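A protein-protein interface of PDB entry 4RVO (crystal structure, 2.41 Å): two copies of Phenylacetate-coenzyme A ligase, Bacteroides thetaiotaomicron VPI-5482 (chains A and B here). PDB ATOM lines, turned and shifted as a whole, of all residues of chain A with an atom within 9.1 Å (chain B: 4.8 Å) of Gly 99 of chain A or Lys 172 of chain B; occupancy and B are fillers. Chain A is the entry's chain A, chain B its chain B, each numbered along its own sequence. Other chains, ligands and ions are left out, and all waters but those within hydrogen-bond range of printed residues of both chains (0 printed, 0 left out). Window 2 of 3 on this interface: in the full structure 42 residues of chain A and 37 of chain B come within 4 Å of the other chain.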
ATOM      1  N   ARG A  72       1.956 -17.125  -8.431  1.00  0.00           N
ATOM      2  CA  ARG A  72       2.530 -15.885  -7.869  1.00  0.00           C
ATOM      3  C   ARG A  72       3.949 -15.660  -8.400  1.00  0.00           C
ATOM      4  O   ARG A  72       4.348 -14.519  -8.638  1.00  0.00           O
ATOM      5  CB  ARG A  72       2.549 -15.935  -6.334  1.00  0.00           C
ATOM      6  CG  ARG A  72       1.176 -15.828  -5.685  1.00  0.00           C
ATOM      7  CD  ARG A  72       1.305 -15.644  -4.188  1.00  0.00           C
ATOM      8  NE  ARG A  72       0.004 -15.593  -3.524  1.00  0.00           N
ATOM      9  CZ  ARG A  72      -0.491 -16.585  -2.795  1.00  0.00           C
ATOM     10  NH1 ARG A  72       0.206 -17.702  -2.621  1.00  0.00           N
ATOM     11  NH2 ARG A  72      -1.676 -16.461  -2.212  1.00  0.00           N
ATOM     12  N   TYR A  75       3.787 -14.245 -11.940  1.00  0.00           N
ATOM     13  CA  TYR A  75       2.924 -13.068 -12.045  1.00  0.00           C
ATOM     14  C   TYR A  75       3.570 -11.992 -12.948  1.00  0.00           C
ATOM     15  O   TYR A  75       4.778 -11.753 -12.857  1.00  0.00           O
ATOM     16  CB  TYR A  75       2.636 -12.494 -10.638  1.00  0.00           C
ATOM     17  CG  TYR A  75       1.867 -11.190 -10.651  1.00  0.00           C
ATOM     18  CD1 TYR A  75       0.476 -11.178 -10.671  1.00  0.00           C
ATOM     19  CD2 TYR A  75       2.528  -9.968 -10.574  1.00  0.00           C
ATOM     20  CE1 TYR A  75      -0.236  -9.982 -10.679  1.00  0.00           C
ATOM     21  CE2 TYR A  75       1.827  -8.765 -10.571  1.00  0.00           C
ATOM     22  CZ  TYR A  75       0.444  -8.775 -10.619  1.00  0.00           C
ATOM     23  OH  TYR A  75      -0.250  -7.591 -10.622  1.00  0.00           O
ATOM     24  N   PRO A  76       2.790 -11.376 -13.884  1.00  0.00           N
ATOM     25  CA  PRO A  76       1.345 -11.510 -14.056  1.00  0.00           C
ATOM     26  C   PRO A  76       0.937 -12.441 -15.227  1.00  0.00           C
ATOM     27  O   PRO A  76      -0.159 -13.005 -15.193  1.00  0.00           O
ATOM     28  CB  PRO A  76       0.906 -10.066 -14.319  1.00  0.00           C
ATOM     29  CG  PRO A  76       2.112  -9.409 -15.021  1.00  0.00           C
ATOM     30  CD  PRO A  76       3.332 -10.272 -14.707  1.00  0.00           C
ATOM     31  N   PHE A  77       1.792 -12.573 -16.275  1.00  0.00           N
ATOM     32  CA  PHE A  77       1.375 -13.257 -17.500  1.00  0.00           C
ATOM     33  C   PHE A  77       2.285 -14.472 -17.861  1.00  0.00           C
ATOM     34  O   PHE A  77       2.276 -14.922 -19.004  1.00  0.00           O
ATOM     35  CB  PHE A  77       1.339 -12.267 -18.672  1.00  0.00           C
ATOM     36  CG  PHE A  77       0.555 -10.998 -18.386  1.00  0.00           C
ATOM     37  CD1 PHE A  77      -0.792 -11.056 -18.037  1.00  0.00           C
ATOM     38  CD2 PHE A  77       1.135  -9.746 -18.568  1.00  0.00           C
ATOM     39  CE1 PHE A  77      -1.521  -9.885 -17.809  1.00  0.00           C
ATOM     40  CE2 PHE A  77       0.403  -8.579 -18.339  1.00  0.00           C
ATOM     41  CZ  PHE A  77      -0.922  -8.657 -17.970  1.00  0.00           C
ATOM     42  N   SER A  93      -8.280 -10.213 -11.557  1.00  0.00           N
ATOM     43  CA  SER A  93      -7.222 -10.242 -10.567  1.00  0.00           C
ATOM     44  C   SER A  93      -7.786 -10.373  -9.150  1.00  0.00           C
ATOM     45  O   SER A  93      -8.807  -9.763  -8.833  1.00  0.00           O
ATOM     46  CB  SER A  93      -6.369  -8.982 -10.671  1.00  0.00           C
ATOM     47  OG  SER A  93      -5.267  -9.032  -9.780  1.00  0.00           O
ATOM     48  N   SER A  94      -7.091 -11.121  -8.281  1.00  0.00           N
ATOM     49  CA  SER A  94      -7.479 -11.203  -6.874  1.00  0.00           C
ATOM     50  C   SER A  94      -6.994  -9.946  -6.116  1.00  0.00           C
ATOM     51  O   SER A  94      -6.306  -9.098  -6.701  1.00  0.00           O
ATOM     52  CB  SER A  94      -6.922 -12.476  -6.228  1.00  0.00           C
ATOM     53  OG  SER A  94      -5.507 -12.471  -6.181  1.00  0.00           O
ATOM     54  N   SER A  95      -7.401  -9.800  -4.848  1.00  0.00           N
ATOM     55  CA  SER A  95      -7.091  -8.612  -4.044  1.00  0.00           C
ATOM     56  C   SER A  95      -5.594  -8.511  -3.710  1.00  0.00           C
ATOM     57  O   SER A  95      -4.888  -9.523  -3.701  1.00  0.00           O
ATOM     58  CB  SER A  95      -7.891  -8.634  -2.749  1.00  0.00           C
ATOM     59  OG  SER A  95      -7.515  -9.733  -1.935  1.00  0.00           O
ATOM     60  N   GLY A  96      -5.154  -7.308  -3.342  1.00  0.00           N
ATOM     61  CA  GLY A  96      -3.847  -7.121  -2.746  1.00  0.00           C
ATOM     62  C   GLY A  96      -2.890  -6.205  -3.478  1.00  0.00           C
ATOM     63  O   GLY A  96      -2.931  -6.090  -4.710  1.00  0.00           O
ATOM     64  N   THR A  97      -1.983  -5.555  -2.691  1.00  0.00           N
ATOM     65  CA  THR A  97      -0.884  -4.737  -3.220  1.00  0.00           C
ATOM     66  C   THR A  97       0.419  -5.089  -2.484  1.00  0.00           C
ATOM     67  O   THR A  97       1.508  -4.765  -2.961  1.00  0.00           O
ATOM     68  CB  THR A  97      -1.211  -3.223  -3.097  1.00  0.00           C
ATOM     69  OG1 THR A  97      -1.608  -2.933  -1.754  1.00  0.00           O
ATOM     70  CG2 THR A  97      -2.293  -2.778  -4.071  1.00  0.00           C
ATOM     71  N   THR A  98       0.301  -5.799  -1.325  1.00  0.00           N
ATOM     72  CA  THR A  98       1.456  -6.213  -0.508  1.00  0.00           C
ATOM     73  C   THR A  98       2.149  -7.467  -1.112  1.00  0.00           C
ATOM     74  O   THR A  98       3.315  -7.740  -0.806  1.00  0.00           O
ATOM     75  CB  THR A  98       1.012  -6.479   0.943  1.00  0.00           C
ATOM     76  OG1 THR A  98       0.022  -7.509   0.949  1.00  0.00           O
ATOM     77  CG2 THR A  98       0.474  -5.230   1.630  1.00  0.00           C
ATOM     78  N   GLY A  99       1.408  -8.221  -1.924  1.00  0.00           N
ATOM     79  CA  GLY A  99       1.933  -9.389  -2.624  1.00  0.00           C
ATOM     80  C   GLY A  99       1.459  -9.464  -4.064  1.00  0.00           C
ATOM     81  O   GLY A  99       0.659  -8.631  -4.498  1.00  0.00           O
ATOM     82  N   ASN A 100       1.956 -10.456  -4.825  1.00  0.00           N
ATOM     83  CA  ASN A 100       1.526 -10.650  -6.212  1.00  0.00           C
ATOM     84  C   ASN A 100       0.183 -11.379  -6.256  1.00  0.00           C
ATOM     85  O   ASN A 100       0.084 -12.534  -5.824  1.00  0.00           O
ATOM     86  CB  ASN A 100       2.584 -11.424  -7.011  1.00  0.00           C
ATOM     87  CG  ASN A 100       3.816 -10.617  -7.331  1.00  0.00           C
ATOM     88  OD1 ASN A 100       3.777  -9.380  -7.436  1.00  0.00           O
ATOM     89  ND2 ASN A 100       4.910 -11.308  -7.613  1.00  0.00           N
ATOM     90  N   PRO A 101      -0.883 -10.719  -6.762  1.00  0.00           N
ATOM     91  CA  PRO A 101      -2.195 -11.371  -6.775  1.00  0.00           C
ATOM     92  C   PRO A 101      -2.315 -12.434  -7.888  1.00  0.00           C
ATOM     93  O   PRO A 101      -1.353 -12.696  -8.616  1.00  0.00           O
ATOM     94  CB  PRO A 101      -3.162 -10.209  -7.005  1.00  0.00           C
ATOM     95  CG  PRO A 101      -2.380  -9.215  -7.752  1.00  0.00           C
ATOM     96  CD  PRO A 101      -0.957  -9.334  -7.274  1.00  0.00           C
ATOM     97  N   THR A 102      -3.481 -13.079  -7.973  1.00  0.00           N
ATOM     98  CA  THR A 102      -3.766 -14.061  -9.007  1.00  0.00           C
ATOM     99  C   THR A 102      -4.341 -13.361 -10.219  1.00  0.00           C
ATOM    100  O   THR A 102      -5.250 -12.553 -10.078  1.00  0.00           O
ATOM    101  CB  THR A 102      -4.738 -15.127  -8.459  1.00  0.00           C
ATOM    102  OG1 THR A 102      -4.198 -15.677  -7.263  1.00  0.00           O
ATOM    103  CG2 THR A 102      -5.022 -16.235  -9.464  1.00  0.00           C
ATOM    104  N   VAL A 103      -3.821 -13.654 -11.402  1.00  0.00           N
ATOM    105  CA  VAL A 103      -4.314 -13.020 -12.615  1.00  0.00           C
ATOM    106  C   VAL A 103      -4.776 -14.089 -13.629  1.00  0.00           C
ATOM    107  O   VAL A 103      -4.041 -15.021 -13.914  1.00  0.00           O
ATOM    108  CB  VAL A 103      -3.248 -12.068 -13.229  1.00  0.00           C
ATOM    109  CG1 VAL A 103      -3.577 -11.730 -14.689  1.00  0.00           C
ATOM    110  CG2 VAL A 103      -3.115 -10.798 -12.395  1.00  0.00           C
ATOM    111  N   MET A 141     -13.491  -6.436 -10.508  1.00  0.00           N
ATOM    112  CA  MET A 141     -12.573  -7.578 -10.613  1.00  0.00           C
ATOM    113  C   MET A 141     -13.212  -8.899 -10.083  1.00  0.00           C
ATOM    114  O   MET A 141     -12.734  -9.983 -10.420  1.00  0.00           O
ATOM    115  CB  MET A 141     -11.262  -7.290  -9.869  1.00  0.00           C
ATOM    116  CG  MET A 141     -10.325  -6.367 -10.638  1.00  0.00           C
ATOM    117  SD  MET A 141      -9.895  -7.079 -12.399  1.00  0.00           S
ATOM    118  CE  MET A 141      -8.452  -5.996 -12.790  1.00  0.00           C
ATOM    119  N   MET A 344      -1.616 -13.353   5.922  1.00  0.00           N
ATOM    120  CA  MET A 344      -0.387 -12.594   5.642  1.00  0.00           C
ATOM    121  C   MET A 344      -0.712 -11.224   5.026  1.00  0.00           C
ATOM    122  O   MET A 344       0.054 -10.283   5.197  1.00  0.00           O
ATOM    123  CB  MET A 344       0.563 -13.389   4.710  1.00  0.00           C
ATOM    124  CG  MET A 344       0.021 -13.575   3.289  1.00  0.00           C
ATOM    125  SD  MET A 344       1.421 -14.089   2.007  1.00  0.00           S
ATOM    126  CE  MET A 344       0.302 -14.302   0.398  1.00  0.00           C
ATOM    127  N   GLN A 345      -1.890 -11.103   4.337  1.00  0.00           N
ATOM    128  CA  GLN A 345      -2.327  -9.812   3.768  1.00  0.00           C
ATOM    129  C   GLN A 345      -2.581  -8.806   4.884  1.00  0.00           C
ATOM    130  O   GLN A 345      -2.288  -7.618   4.728  1.00  0.00           O
ATOM    131  CB  GLN A 345      -3.598  -9.983   2.914  1.00  0.00           C
ATOM    132  CG  GLN A 345      -3.381 -10.743   1.620  1.00  0.00           C
ATOM    133  CD  GLN A 345      -4.645 -10.777   0.795  1.00  0.00           C
ATOM    134  OE1 GLN A 345      -5.532 -11.621   0.997  1.00  0.00           O
ATOM    135  NE2 GLN A 345      -4.784  -9.817  -0.116  1.00  0.00           N
ATOM    136  N   LYS A 348       1.027  -7.992   6.555  1.00  0.00           N
ATOM    137  CA  LYS A 348       1.846  -7.134   5.680  1.00  0.00           C
ATOM    138  C   LYS A 348       1.408  -5.651   5.767  1.00  0.00           C
ATOM    139  O   LYS A 348       2.215  -4.755   5.510  1.00  0.00           O
ATOM    140  CB  LYS A 348       1.787  -7.627   4.230  1.00  0.00           C
ATOM    141  CG  LYS A 348       2.641  -8.875   3.989  1.00  0.00           C
ATOM    142  CD  LYS A 348       2.468  -9.433   2.583  1.00  0.00           C
ATOM    143  CE  LYS A 348       3.288 -10.685   2.372  1.00  0.00           C
ATOM    144  NZ  LYS A 348       3.108 -11.237   1.003  1.00  0.00           N
ATOM    145  N   ILE A 349       0.141  -5.401   6.178  1.00  0.00           N
ATOM    146  CA  ILE A 349      -0.364  -4.043   6.386  1.00  0.00           C
ATOM    147  C   ILE A 349       0.014  -3.550   7.812  1.00  0.00           C
ATOM    148  O   ILE A 349       0.498  -2.427   7.964  1.00  0.00           O
ATOM    149  CB  ILE A 349      -1.916  -3.982   6.147  1.00  0.00           C
ATOM    150  CG1 ILE A 349      -2.286  -4.370   4.674  1.00  0.00           C
ATOM    151  CG2 ILE A 349      -2.494  -2.596   6.530  1.00  0.00           C
ATOM    152  CD1 ILE A 349      -1.879  -3.278   3.548  1.00  0.00           C
ATOM    153  N   GLN A 352       3.602  -2.179   8.719  1.00  0.00           N
ATOM    154  CA  GLN A 352       3.927  -0.837   8.202  1.00  0.00           C
ATOM    155  C   GLN A 352       3.727   0.256   9.285  1.00  0.00           C
ATOM    156  O   GLN A 352       4.240   1.367   9.135  1.00  0.00           O
ATOM    157  CB  GLN A 352       3.079  -0.515   6.961  1.00  0.00           C
ATOM    158  CG  GLN A 352       3.715  -0.995   5.653  1.00  0.00           C
ATOM    159  CD  GLN A 352       2.718  -1.049   4.532  1.00  0.00           C
ATOM    160  OE1 GLN A 352       2.387  -0.034   3.907  1.00  0.00           O
ATOM    161  NE2 GLN A 352       2.243  -2.243   4.223  1.00  0.00           N
ATOM    162  N   GLU A 404      -6.775  -3.402   0.974  1.00  0.00           N
ATOM    163  CA  GLU A 404      -5.989  -4.606   0.704  1.00  0.00           C
ATOM    164  C   GLU A 404      -6.885  -5.865   0.590  1.00  0.00           C
ATOM    165  O   GLU A 404      -6.767  -6.609  -0.385  1.00  0.00           O
ATOM    166  CB  GLU A 404      -4.921  -4.811   1.803  1.00  0.00           C
ATOM    167  CG  GLU A 404      -4.098  -6.096   1.643  1.00  0.00           C
ATOM    168  CD  GLU A 404      -3.087  -6.095   0.505  1.00  0.00           C
ATOM    169  OE1 GLU A 404      -2.779  -5.000  -0.022  1.00  0.00           O
ATOM    170  OE2 GLU A 404      -2.543  -7.180   0.200  1.00  0.00           O
ATOM    171  N   LYS B 168      -4.251   2.866  -4.926  1.00  0.00           N
ATOM    172  CA  LYS B 168      -3.044   2.019  -4.875  1.00  0.00           C
ATOM    173  C   LYS B 168      -3.191   0.799  -5.795  1.00  0.00           C
ATOM    174  O   LYS B 168      -2.222   0.392  -6.435  1.00  0.00           O
ATOM    175  CB  LYS B 168      -2.749   1.563  -3.430  1.00  0.00           C
ATOM    176  CG  LYS B 168      -2.259   2.688  -2.524  1.00  0.00           C
ATOM    177  CD  LYS B 168      -1.909   2.178  -1.131  1.00  0.00           C
ATOM    178  CE  LYS B 168      -1.442   3.292  -0.228  1.00  0.00           C
ATOM    179  NZ  LYS B 168      -1.051   2.785   1.113  1.00  0.00           N
ATOM    180  N   ARG B 169      -4.414   0.236  -5.879  1.00  0.00           N
ATOM    181  CA  ARG B 169      -4.689  -0.917  -6.734  1.00  0.00           C
ATOM    182  C   ARG B 169      -4.779  -0.479  -8.203  1.00  0.00           C
ATOM    183  O   ARG B 169      -4.296  -1.191  -9.090  1.00  0.00           O
ATOM    184  CB  ARG B 169      -5.993  -1.609  -6.292  1.00  0.00           C
ATOM    185  CG  ARG B 169      -6.061  -3.085  -6.642  1.00  0.00           C
ATOM    186  CD  ARG B 169      -7.411  -3.670  -6.255  1.00  0.00           C
ATOM    187  NE  ARG B 169      -7.527  -5.080  -6.625  1.00  0.00           N
ATOM    188  CZ  ARG B 169      -8.685  -5.729  -6.708  1.00  0.00           C
ATOM    189  NH1 ARG B 169      -9.828  -5.090  -6.490  1.00  0.00           N
ATOM    190  NH2 ARG B 169      -8.712  -7.012  -7.041  1.00  0.00           N
ATOM    191  N   GLN B 170      -5.360   0.720  -8.454  1.00  0.00           N
ATOM    192  CA  GLN B 170      -5.439   1.301  -9.810  1.00  0.00           C
ATOM    193  C   GLN B 170      -4.039   1.473 -10.395  1.00  0.00           C
ATOM    194  O   GLN B 170      -3.799   1.095 -11.538  1.00  0.00           O
ATOM    195  CB  GLN B 170      -6.172   2.667  -9.778  1.00  0.00           C
ATOM    196  CG  GLN B 170      -7.612   2.600  -9.255  1.00  0.00           C
ATOM    197  CD  GLN B 170      -8.609   2.179 -10.315  1.00  0.00           C
ATOM    198  OE1 GLN B 170      -8.275   2.014 -11.503  1.00  0.00           O
ATOM    199  NE2 GLN B 170      -9.877   2.072  -9.922  1.00  0.00           N
ATOM    200  N   ILE B 171      -3.101   2.032  -9.587  1.00  0.00           N
ATOM    201  CA  ILE B 171      -1.716   2.279 -10.002  1.00  0.00           C
ATOM    202  C   ILE B 171      -0.980   0.942 -10.210  1.00  0.00           C
ATOM    203  O   ILE B 171      -0.179   0.817 -11.144  1.00  0.00           O
ATOM    204  CB  ILE B 171      -0.984   3.193  -8.941  1.00  0.00           C
ATOM    205  CG1 ILE B 171      -1.229   4.689  -9.230  1.00  0.00           C
ATOM    206  CG2 ILE B 171       0.519   2.896  -8.885  1.00  0.00           C
ATOM    207  CD1 ILE B 171      -2.597   5.138  -9.051  1.00  0.00           C
ATOM    208  N   LYS B 172      -1.283  -0.064  -9.363  1.00  0.00           N
ATOM    209  CA  LYS B 172      -0.678  -1.390  -9.484  1.00  0.00           C
ATOM    210  C   LYS B 172      -1.088  -2.052 -10.804  1.00  0.00           C
ATOM    211  O   LYS B 172      -0.242  -2.621 -11.492  1.00  0.00           O
ATOM    212  CB  LYS B 172      -1.069  -2.282  -8.292  1.00  0.00           C
ATOM    213  CG  LYS B 172      -0.425  -3.658  -8.345  1.00  0.00           C
ATOM    214  CD  LYS B 172      -0.629  -4.431  -7.073  1.00  0.00           C
ATOM    215  CE  LYS B 172       0.078  -5.775  -7.112  1.00  0.00           C
ATOM    216  NZ  LYS B 172       1.558  -5.629  -7.275  1.00  0.00           N
ATOM    217  N   PHE B 173      -2.383  -1.937 -11.177  1.00  0.00           N
ATOM    218  CA  PHE B 173      -2.881  -2.490 -12.437  1.00  0.00           C
ATOM    219  C   PHE B 173      -2.187  -1.832 -13.639  1.00  0.00           C
ATOM    220  O   PHE B 173      -1.725  -2.535 -14.539  1.00  0.00           O
ATOM    221  CB  PHE B 173      -4.412  -2.318 -12.549  1.00  0.00           C
ATOM    222  CG  PHE B 173      -5.219  -3.101 -11.539  1.00  0.00           C
ATOM    223  CD1 PHE B 173      -4.693  -4.240 -10.936  1.00  0.00           C
ATOM    224  CD2 PHE B 173      -6.550  -2.777 -11.287  1.00  0.00           C
ATOM    225  CE1 PHE B 173      -5.457  -4.991 -10.039  1.00  0.00           C
ATOM    226  CE2 PHE B 173      -7.315  -3.533 -10.395  1.00  0.00           C
ATOM    227  CZ  PHE B 173      -6.771  -4.647  -9.793  1.00  0.00           C
ATOM    228  N   ILE B 174      -2.079  -0.479 -13.634  1.00  0.00           N
ATOM    229  CA  ILE B 174      -1.427   0.265 -14.730  1.00  0.00           C
ATOM    230  C   ILE B 174       0.044  -0.186 -14.887  1.00  0.00           C
ATOM    231  O   ILE B 174       0.499  -0.415 -16.004  1.00  0.00           O
ATOM    232  CB  ILE B 174      -1.528   1.810 -14.495  1.00  0.00           C
ATOM    233  CG1 ILE B 174      -3.008   2.282 -14.555  1.00  0.00           C
ATOM    234  CG2 ILE B 174      -0.661   2.580 -15.508  1.00  0.00           C
ATOM    235  CD1 ILE B 174      -3.244   3.712 -14.030  1.00  0.00           C
ATOM    236  N   SER B 175       0.759  -0.350 -13.760  1.00  0.00           N
ATOM    237  CA  SER B 175       2.180  -0.713 -13.775  1.00  0.00           C
ATOM    238  C   SER B 175       2.391  -2.178 -14.213  1.00  0.00           C
ATOM    239  O   SER B 175       3.272  -2.455 -15.025  1.00  0.00           O
ATOM    240  CB  SER B 175       2.796  -0.495 -12.396  1.00  0.00           C
ATOM    241  OG  SER B 175       2.561   0.822 -11.927  1.00  0.00           O
ATOM    242  N   ASP B 176       1.591  -3.115 -13.651  1.00  0.00           N
ATOM    243  CA  ASP B 176       1.777  -4.548 -13.878  1.00  0.00           C
ATOM    244  C   ASP B 176       1.158  -5.011 -15.210  1.00  0.00           C
ATOM    245  O   ASP B 176       1.714  -5.889 -15.859  1.00  0.00           O
ATOM    246  CB  ASP B 176       1.176  -5.357 -12.714  1.00  0.00           C
ATOM    247  CG  ASP B 176       1.843  -5.083 -11.364  1.00  0.00           C
ATOM    248  OD1 ASP B 176       2.916  -4.433 -11.350  1.00  0.00           O
ATOM    249  OD2 ASP B 176       1.322  -5.563 -10.341  1.00  0.00           O
ATOM    250  N   PHE B 177      -0.029  -4.479 -15.573  1.00  0.00           N
ATOM    251  CA  PHE B 177      -0.729  -4.932 -16.790  1.00  0.00           C
ATOM    252  C   PHE B 177      -0.388  -4.046 -17.993  1.00  0.00           C
ATOM    253  O   PHE B 177      -0.856  -4.315 -19.103  1.00  0.00           O
ATOM    254  CB  PHE B 177      -2.259  -4.960 -16.568  1.00  0.00           C
ATOM    255  CG  PHE B 177      -2.705  -5.718 -15.336  1.00  0.00           C
ATOM    256  CD1 PHE B 177      -1.997  -6.832 -14.888  1.00  0.00           C
ATOM    257  CD2 PHE B 177      -3.887  -5.384 -14.686  1.00  0.00           C
ATOM    258  CE1 PHE B 177      -2.404  -7.523 -13.747  1.00  0.00           C
ATOM    259  CE2 PHE B 177      -4.324  -6.113 -13.582  1.00  0.00           C
ATOM    260  CZ  PHE B 177      -3.574  -7.171 -13.109  1.00  0.00           C
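OD2 of Asp 176 of chain B lies within hydrogen-bond range of OH of Tyr 75 of chain A, 2.6 Å away.
The backbone carbonyl oxygen of Ser 94 of chain A sits at hydrogen-bond distance from the guanidinium group of Arg 169 of chain B (3.2 Å).
The backbone carbonyl oxygen (O) of Ser 93 of chain A sits at hydrogen-bond distance from the guanidinium group (NH2) of Arg 169 of chain B (3.3 Å).
The side-chain carboxylate (OD2) of Asp 176 of chain B is in salt-bridge range of the side-chain amino group (NZ) of Lys 172 of chain B.
The backbone NH of Gly 96 of chain A is in hydrogen-bond range of the backbone carbonyl oxygen of Glu 404 of chain A, 3.4 Å away.
OG of Ser 95 of chain A lies within hydrogen-bond range of NE2 of Gln 345 of chain A, 3.3 Å away.
The backbone NH of Thr 97 of chain A lies within hydrogen-bond range of the side-chain carboxylate of Glu 404 of chain A (2.8 Å).
N of Thr 102 of chain A is in hydrogen-bond range of OG of Ser 94 of chain A (2.8 Å).
N of Ser 93 of chain A is in hydrogen-bond range of SD of Met 141 of chain A, at 3.6 Å.
Among the printed residues, pairs that only touch across the chains: Val 103 of chain A with Phe 177 of chain B, Met 141 of chain A with Phe 173 of chain B, Pro 76 of chain A with Asp 176 of chain B, Gly 96 of chain A with Lys 172 of chain B, Pro 101 of chain A with Lys 172 of chain B, Phe 77 of chain A with Phe 177 of chain B, Ser 95 of chain A with Arg 169 of chain B, Tyr 75 of chain A with Phe 177 of chain B, Thr 97 of chain A with Lys 172 of chain B, Met 141 of chain A with Arg 169 of chain B, Phe 77 of chain A with Asp 176 of chain B, Gly 99 of chain A with Lys 172 of chain B, Thr 97 of chain A with Lys 168 of chain B and Tyr 75 of chain A with Lys 172 of chain B.
Printed residues of chain B within 4 Å of Ser 94 of chain A: Arg 169.
Of the printed residues of chain B, Ser 95 of chain A touches Arg 169 (3.8 Å).
Of the printed residues of chain B, Thr 97 of chain A touches Lys 168 and Lys 172.
Met 344 of chain A touches none of the printed residues of chain B.
Of the printed residues of chain A, Lys 172 of chain B touches Tyr 75, Gly 96, Thr 97, Gly 99 and Pro 101.
The nearest printed residue of chain B that does not touch Pro 76 of chain A is Phe 177 of chain B (4.2 Å).
Of the 10 printed residues of chain B, 6 touch a printed residue of chain A.
Hydrophobic or aromatic side chains of chain B that line the printed part of chain A: Phe 173 and Phe 177.
Hydrophobic or aromatic side chains of chain A within 4 Å of the printed part of chain B: Tyr 75, Pro 76, Phe 77, Pro 101, Val 103 and Met 141.
Among the printed residues, 17 pairs touch across the chains.
Among the printed residues, no Asp or Glu carboxylate lies within 4 Å of a Lys or Arg side-chain nitrogen of the other chain.
No position is printed for both chains.
Of the 17 pairs that touch across the chains among the printed residues, none has its exchanged pair printed and touching as well.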
